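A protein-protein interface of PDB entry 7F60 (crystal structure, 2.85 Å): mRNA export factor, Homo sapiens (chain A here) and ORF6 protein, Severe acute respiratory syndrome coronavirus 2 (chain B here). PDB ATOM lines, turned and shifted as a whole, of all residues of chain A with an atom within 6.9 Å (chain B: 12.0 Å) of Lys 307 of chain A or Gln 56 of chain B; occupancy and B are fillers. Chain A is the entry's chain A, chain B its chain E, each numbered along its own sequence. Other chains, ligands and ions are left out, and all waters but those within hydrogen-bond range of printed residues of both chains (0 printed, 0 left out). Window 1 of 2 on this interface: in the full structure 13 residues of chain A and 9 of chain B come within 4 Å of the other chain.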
ATOM      1  N   SER A 298     -21.260  -6.815  22.040  1.00  0.00           N
ATOM      2  CA  SER A 298     -22.554  -6.170  22.204  1.00  0.00           C
ATOM      3  C   SER A 298     -22.619  -5.439  23.536  1.00  0.00           C
ATOM      4  O   SER A 298     -22.002  -5.851  24.520  1.00  0.00           O
ATOM      5  CB  SER A 298     -23.701  -7.185  22.112  1.00  0.00           C
ATOM      6  OG  SER A 298     -23.944  -7.552  20.768  1.00  0.00           O
ATOM      7  N   PHE A 299     -23.374  -4.347  23.555  1.00  0.00           N
ATOM      8  CA  PHE A 299     -23.657  -3.611  24.777  1.00  0.00           C
ATOM      9  C   PHE A 299     -25.090  -3.894  25.207  1.00  0.00           C
ATOM     10  O   PHE A 299     -25.995  -3.965  24.373  1.00  0.00           O
ATOM     11  CB  PHE A 299     -23.449  -2.108  24.580  1.00  0.00           C
ATOM     12  CG  PHE A 299     -22.052  -1.731  24.182  1.00  0.00           C
ATOM     13  CD1 PHE A 299     -20.971  -2.523  24.527  1.00  0.00           C
ATOM     14  CD2 PHE A 299     -21.823  -0.570  23.463  1.00  0.00           C
ATOM     15  CE1 PHE A 299     -19.689  -2.167  24.163  1.00  0.00           C
ATOM     16  CE2 PHE A 299     -20.546  -0.209  23.095  1.00  0.00           C
ATOM     17  CZ  PHE A 299     -19.477  -1.008  23.445  1.00  0.00           C
ATOM     18  N   TRP A 300     -25.289  -4.053  26.513  1.00  0.00           N
ATOM     19  CA  TRP A 300     -26.567  -4.468  27.069  1.00  0.00           C
ATOM     20  C   TRP A 300     -26.942  -3.601  28.260  1.00  0.00           C
ATOM     21  O   TRP A 300     -26.080  -3.044  28.941  1.00  0.00           O
ATOM     22  CB  TRP A 300     -26.539  -5.940  27.507  1.00  0.00           C
ATOM     23  CG  TRP A 300     -26.066  -6.880  26.449  1.00  0.00           C
ATOM     24  CD1 TRP A 300     -24.775  -7.218  26.166  1.00  0.00           C
ATOM     25  CD2 TRP A 300     -26.882  -7.610  25.534  1.00  0.00           C
ATOM     26  NE1 TRP A 300     -24.737  -8.114  25.126  1.00  0.00           N
ATOM     27  CE2 TRP A 300     -26.021  -8.370  24.719  1.00  0.00           C
ATOM     28  CE3 TRP A 300     -28.259  -7.690  25.321  1.00  0.00           C
ATOM     29  CZ2 TRP A 300     -26.493  -9.201  23.710  1.00  0.00           C
ATOM     30  CZ3 TRP A 300     -28.728  -8.517  24.325  1.00  0.00           C
ATOM     31  CH2 TRP A 300     -27.849  -9.261  23.528  1.00  0.00           C
ATOM     32  N   ASP A 301     -28.247  -3.490  28.489  1.00  0.00           N
ATOM     33  CA  ASP A 301     -28.817  -2.873  29.679  1.00  0.00           C
ATOM     34  C   ASP A 301     -29.651  -3.934  30.373  1.00  0.00           C
ATOM     35  O   ASP A 301     -30.599  -4.459  29.778  1.00  0.00           O
ATOM     36  CB  ASP A 301     -29.667  -1.653  29.314  1.00  0.00           C
ATOM     37  CG  ASP A 301     -30.164  -0.885  30.531  1.00  0.00           C
ATOM     38  OD1 ASP A 301     -29.929  -1.333  31.677  1.00  0.00           O
ATOM     39  OD2 ASP A 301     -30.789   0.182  30.326  1.00  0.00           O
ATOM     40  N   ARG A 305     -33.484  -4.195  30.273  1.00  0.00           N
ATOM     41  CA  ARG A 305     -33.530  -5.466  29.548  1.00  0.00           C
ATOM     42  C   ARG A 305     -33.644  -5.216  28.041  1.00  0.00           C
ATOM     43  O   ARG A 305     -34.649  -5.518  27.397  1.00  0.00           O
ATOM     44  CB  ARG A 305     -34.678  -6.358  30.048  1.00  0.00           C
ATOM     45  CG  ARG A 305     -34.818  -6.411  31.559  1.00  0.00           C
ATOM     46  CD  ARG A 305     -35.723  -7.556  31.998  1.00  0.00           C
ATOM     47  NE  ARG A 305     -35.920  -7.536  33.443  1.00  0.00           N
ATOM     48  CZ  ARG A 305     -36.314  -8.581  34.160  1.00  0.00           C
ATOM     49  NH1 ARG A 305     -36.548  -9.737  33.561  1.00  0.00           N
ATOM     50  NH2 ARG A 305     -36.467  -8.472  35.473  1.00  0.00           N
ATOM     51  N   THR A 306     -32.570  -4.648  27.498  1.00  0.00           N
ATOM     52  CA  THR A 306     -32.540  -4.234  26.104  1.00  0.00           C
ATOM     53  C   THR A 306     -31.136  -4.393  25.539  1.00  0.00           C
ATOM     54  O   THR A 306     -30.141  -4.347  26.270  1.00  0.00           O
ATOM     55  CB  THR A 306     -33.002  -2.785  25.940  1.00  0.00           C
ATOM     56  OG1 THR A 306     -33.251  -2.525  24.551  1.00  0.00           O
ATOM     57  CG2 THR A 306     -31.934  -1.826  26.457  1.00  0.00           C
ATOM     58  N   LYS A 307     -31.069  -4.577  24.224  1.00  0.00           N
ATOM     59  CA  LYS A 307     -29.802  -4.677  23.516  1.00  0.00           C
ATOM     60  C   LYS A 307     -29.460  -3.309  22.935  1.00  0.00           C
ATOM     61  O   LYS A 307     -30.204  -2.780  22.101  1.00  0.00           O
ATOM     62  CB  LYS A 307     -29.891  -5.743  22.422  1.00  0.00           C
ATOM     63  CG  LYS A 307     -28.549  -6.145  21.820  1.00  0.00           C
ATOM     64  CD  LYS A 307     -28.166  -5.217  20.686  1.00  0.00           C
ATOM     65  CE  LYS A 307     -29.149  -5.321  19.529  1.00  0.00           C
ATOM     66  NZ  LYS A 307     -29.145  -4.095  18.673  1.00  0.00           N
ATOM     67  N   LEU A 308     -28.333  -2.742  23.363  1.00  0.00           N
ATOM     68  CA  LEU A 308     -27.996  -1.389  22.936  1.00  0.00           C
ATOM     69  C   LEU A 308     -27.332  -1.383  21.564  1.00  0.00           C
ATOM     70  O   LEU A 308     -27.746  -0.632  20.674  1.00  0.00           O
ATOM     71  CB  LEU A 308     -27.107  -0.721  23.983  1.00  0.00           C
ATOM     72  CG  LEU A 308     -27.755  -0.529  25.356  1.00  0.00           C
ATOM     73  CD1 LEU A 308     -26.756   0.063  26.328  1.00  0.00           C
ATOM     74  CD2 LEU A 308     -28.997   0.350  25.253  1.00  0.00           C
ATOM     75  N   LYS A 309     -26.317  -2.222  21.367  1.00  0.00           N
ATOM     76  CA  LYS A 309     -25.595  -2.246  20.105  1.00  0.00           C
ATOM     77  C   LYS A 309     -25.054  -3.643  19.844  1.00  0.00           C
ATOM     78  O   LYS A 309     -24.917  -4.462  20.756  1.00  0.00           O
ATOM     79  CB  LYS A 309     -24.444  -1.231  20.094  1.00  0.00           C
ATOM     80  CG  LYS A 309     -24.846   0.180  19.706  1.00  0.00           C
ATOM     81  CD  LYS A 309     -23.625   1.071  19.546  1.00  0.00           C
ATOM     82  CE  LYS A 309     -22.698   0.550  18.458  1.00  0.00           C
ATOM     83  NZ  LYS A 309     -23.358   0.559  17.124  1.00  0.00           N
ATOM     84  N   THR A 310     -24.749  -3.900  18.574  1.00  0.00           N
ATOM     85  CA  THR A 310     -24.020  -5.086  18.146  1.00  0.00           C
ATOM     86  C   THR A 310     -23.131  -4.690  16.979  1.00  0.00           C
ATOM     87  O   THR A 310     -23.576  -3.996  16.060  1.00  0.00           O
ATOM     88  CB  THR A 310     -24.959  -6.230  17.737  1.00  0.00           C
ATOM     89  OG1 THR A 310     -25.853  -6.530  18.816  1.00  0.00           O
ATOM     90  CG2 THR A 310     -24.155  -7.481  17.398  1.00  0.00           C
ATOM     91  N   ASP B  53     -26.871  -1.611  16.520  1.00  0.00           N
ATOM     92  CA  ASP B  53     -27.440  -0.480  15.792  1.00  0.00           C
ATOM     93  C   ASP B  53     -28.333   0.341  16.716  1.00  0.00           C
ATOM     94  O   ASP B  53     -27.837   1.066  17.577  1.00  0.00           O
ATOM     95  CB  ASP B  53     -28.229  -0.954  14.564  1.00  0.00           C
ATOM     96  CG  ASP B  53     -28.512  -2.442  14.585  1.00  0.00           C
ATOM     97  OD1 ASP B  53     -27.648  -3.198  15.072  1.00  0.00           O
ATOM     98  OD2 ASP B  53     -29.592  -2.861  14.109  1.00  0.00           O
ATOM     99  N   GLU B  54     -29.644   0.231  16.529  1.00  0.00           N
ATOM    100  CA  GLU B  54     -30.610   0.886  17.397  1.00  0.00           C
ATOM    101  C   GLU B  54     -31.047  -0.061  18.511  1.00  0.00           C
ATOM    102  O   GLU B  54     -30.764  -1.261  18.498  1.00  0.00           O
ATOM    103  CB  GLU B  54     -31.819   1.362  16.597  1.00  0.00           C
ATOM    104  CG  GLU B  54     -32.400   0.297  15.693  1.00  0.00           C
ATOM    105  CD  GLU B  54     -33.874   0.498  15.447  1.00  0.00           C
ATOM    106  OE1 GLU B  54     -34.503  -0.417  14.881  1.00  0.00           O
ATOM    107  OE2 GLU B  54     -34.406   1.566  15.827  1.00  0.00           O
ATOM    108  N   GLU B  55     -31.755   0.503  19.483  1.00  0.00           N
ATOM    109  CA  GLU B  55     -32.148  -0.241  20.671  1.00  0.00           C
ATOM    110  C   GLU B  55     -33.154  -1.329  20.327  1.00  0.00           C
ATOM    111  O   GLU B  55     -34.098  -1.105  19.564  1.00  0.00           O
ATOM    112  CB  GLU B  55     -32.750   0.711  21.704  1.00  0.00           C
ATOM    113  CG  GLU B  55     -32.498   0.321  23.154  1.00  0.00           C
ATOM    114  CD  GLU B  55     -33.051   1.334  24.153  1.00  0.00           C
ATOM    115  OE1 GLU B  55     -33.229   0.941  25.322  1.00  0.00           O
ATOM    116  OE2 GLU B  55     -33.300   2.509  23.786  1.00  0.00           O
ATOM    117  N   GLN B  56     -32.947  -2.509  20.900  1.00  0.00           N
ATOM    118  CA  GLN B  56     -33.830  -3.653  20.763  1.00  0.00           C
ATOM    119  C   GLN B  56     -34.083  -4.266  22.137  1.00  0.00           C
ATOM    120  O   GLN B  56     -33.195  -4.268  22.989  1.00  0.00           O
ATOM    121  CB  GLN B  56     -33.237  -4.730  19.841  1.00  0.00           C
ATOM    122  CG  GLN B  56     -33.047  -4.319  18.390  1.00  0.00           C
ATOM    123  CD  GLN B  56     -32.339  -5.388  17.567  1.00  0.00           C
ATOM    124  OE1 GLN B  56     -31.426  -5.084  16.801  1.00  0.00           O
ATOM    125  NE2 GLN B  56     -32.764  -6.642  17.714  1.00  0.00           N
ATOM    126  N   PRO B  57     -35.280  -4.794  22.359  1.00  0.00           N
ATOM    127  CA  PRO B  57     -35.566  -5.456  23.642  1.00  0.00           C
ATOM    128  C   PRO B  57     -34.842  -6.790  23.772  1.00  0.00           C
ATOM    129  O   PRO B  57     -34.608  -7.492  22.789  1.00  0.00           O
ATOM    130  CB  PRO B  57     -37.088  -5.637  23.605  1.00  0.00           C
ATOM    131  CG  PRO B  57     -37.438  -5.644  22.130  1.00  0.00           C
ATOM    132  CD  PRO B  57     -36.451  -4.729  21.469  1.00  0.00           C
ATOM    133  N   MET B  58     -34.500  -7.150  25.008  1.00  0.00           N
ATOM    134  CA  MET B  58     -33.718  -8.362  25.226  1.00  0.00           C
ATOM    135  C   MET B  58     -34.537  -9.609  24.914  1.00  0.00           C
ATOM    136  O   MET B  58     -35.760  -9.630  25.060  1.00  0.00           O
ATOM    137  CB  MET B  58     -33.208  -8.432  26.664  1.00  0.00           C
ATOM    138  CG  MET B  58     -31.773  -7.979  26.844  1.00  0.00           C
ATOM    139  SD  MET B  58     -31.296  -8.238  28.558  1.00  0.00           S
ATOM    140  CE  MET B  58     -29.667  -7.503  28.583  1.00  0.00           C
ATOM    141  N   GLU B  59     -33.845 -10.656  24.467  1.00  0.00           N
ATOM    142  CA  GLU B  59     -34.477 -11.959  24.257  1.00  0.00           C
ATOM    143  C   GLU B  59     -34.251 -12.758  25.535  1.00  0.00           C
ATOM    144  O   GLU B  59     -33.236 -13.436  25.696  1.00  0.00           O
ATOM    145  CB  GLU B  59     -33.909 -12.663  23.029  1.00  0.00           C
ATOM    146  CG  GLU B  59     -33.352 -11.754  21.952  1.00  0.00           C
ATOM    147  CD  GLU B  59     -31.918 -11.349  22.220  1.00  0.00           C
ATOM    148  OE1 GLU B  59     -31.491 -11.434  23.392  1.00  0.00           O
ATOM    149  OE2 GLU B  59     -31.215 -10.964  21.265  1.00  0.00           O
ATOM    150  N   ILE B  60     -35.212 -12.671  26.457  1.00  0.00           N
ATOM    151  CA  ILE B  60     -35.095 -13.242  27.798  1.00  0.00           C
ATOM    152  C   ILE B  60     -35.995 -14.465  27.919  1.00  0.00           C
ATOM    153  O   ILE B  60     -37.087 -14.521  27.343  1.00  0.00           O
ATOM    154  CB  ILE B  60     -35.437 -12.188  28.881  1.00  0.00           C
ATOM    155  CG1 ILE B  60     -36.222 -12.791  30.062  1.00  0.00           C
ATOM    156  CG2 ILE B  60     -36.161 -10.991  28.259  1.00  0.00           C
ATOM    157  CD1 ILE B  60     -37.728 -12.548  30.036  1.00  0.00           C
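The backbone carbonyl oxygen of Gln 56 of chain B lies within hydrogen-bond range of the backbone NH of Lys 307 of chain A, at 2.5 Å. The side-chain hydroxyl of Thr 306 of chain A lies close to the backbone carbonyl oxygen of Gln 56 of chain B (2.3 Å). The side-chain amino group of Lys 307 of chain A sits at hydrogen-bond distance from the backbone carbonyl oxygen of Glu 54 of chain B (3.3 Å). The backbone carbonyl oxygen (O) of Arg 305 of chain A lies within hydrogen-bond range of the backbone NH (N) of Met 58 of chain B, at 2.9 Å.
Printed residues of chain B within 4 Å of Lys 307 of chain A: Asp 53, Glu 54, Glu 55 and Gln 56. Of chain A, only Thr 306 and Lys 307 come within 4 Å of Gln 56 of chain B. Ser 298 of chain A touches none of the printed residues of chain B. Trp 300 of chain A touches one residue of chain B. Leu 308 of chain A touches just these residues of chain B: Asp 53 and Glu 54. Of chain B, only Asp 53 (3.8 Å) comes within 4 Å of Lys 309 of chain A. Thr 310 of chain A touches just one residue of chain B: Asp 53. Printed residues of chain A within 4 Å of Glu 55 of chain B: Thr 306 (3.3 Å) and Lys 307 (3.5 Å). Of the printed residues of chain A, Asp 53 of chain B touches Lys 307 (3.997 Å), Leu 308 (3.5 Å), Lys 309 (3.8 Å) and Thr 310 (3.7 Å). Ile 60 of chain B touches none of the printed residues of chain A. Glu 59 of chain B touches none of the printed residues of chain A. The nearest printed residue of chain B that does not touch Lys 307 of chain A is Met 58 of chain B (4.4 Å).
The backbone NH (N) of Phe 299 of chain A is in hydrogen-bond range of the backbone carbonyl oxygen (O) of Lys 309 of chain A, at 3.2 Å. The backbone carbonyl oxygen (O) of Asp 301 of chain A lies within hydrogen-bond range of the backbone NH (N) of Thr 306 of chain A (3.0 Å). O of Phe 299 of chain A sits at hydrogen-bond distance from N of Leu 308 of chain A. OG1 of Thr 310 of chain A is in hydrogen-bond range of OG of Ser 298 of chain A (2.9 Å). The side-chain hydroxyl (OG) of Ser 298 of chain A lies within hydrogen-bond range of the backbone carbonyl oxygen (O) of Lys 309 of chain A, 3.2 Å away.
Of the 10 printed residues of chain A, 8 touch a printed residue of chain B. Of the 8 printed residues of chain B, 6 touch a printed residue of chain A. Printed residues of chain B that touch a printed residue of chain A: Asp 53, Glu 54, Glu 55, Gln 56, Pro 57 and Met 58.
Among the printed residues, pairs that only touch across the chains: Trp 300 of chain A with Met 58 of chain B (3.6 Å), Asp 301 of chain A with Met 58 of chain B (3.4 Å), Arg 305 of chain A with Pro 57 of chain B (3.8 Å), Thr 306 of chain A with Glu 55 of chain B (3.3 Å), Thr 306 of chain A with Pro 57 of chain B (3.8 Å), Thr 306 of chain A with Met 58 of chain B (3.5 Å), Lys 307 of chain A with Asp 53 of chain B (3.997 Å), Lys 307 of chain A with Glu 55 of chain B (3.5 Å), Leu 308 of chain A with Asp 53 of chain B (3.5 Å), Leu 308 of chain A with Glu 54 of chain B (3.8 Å), Lys 309 of chain A with Asp 53 of chain B (3.8 Å) and Thr 310 of chain A with Asp 53 of chain B (3.7 Å).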
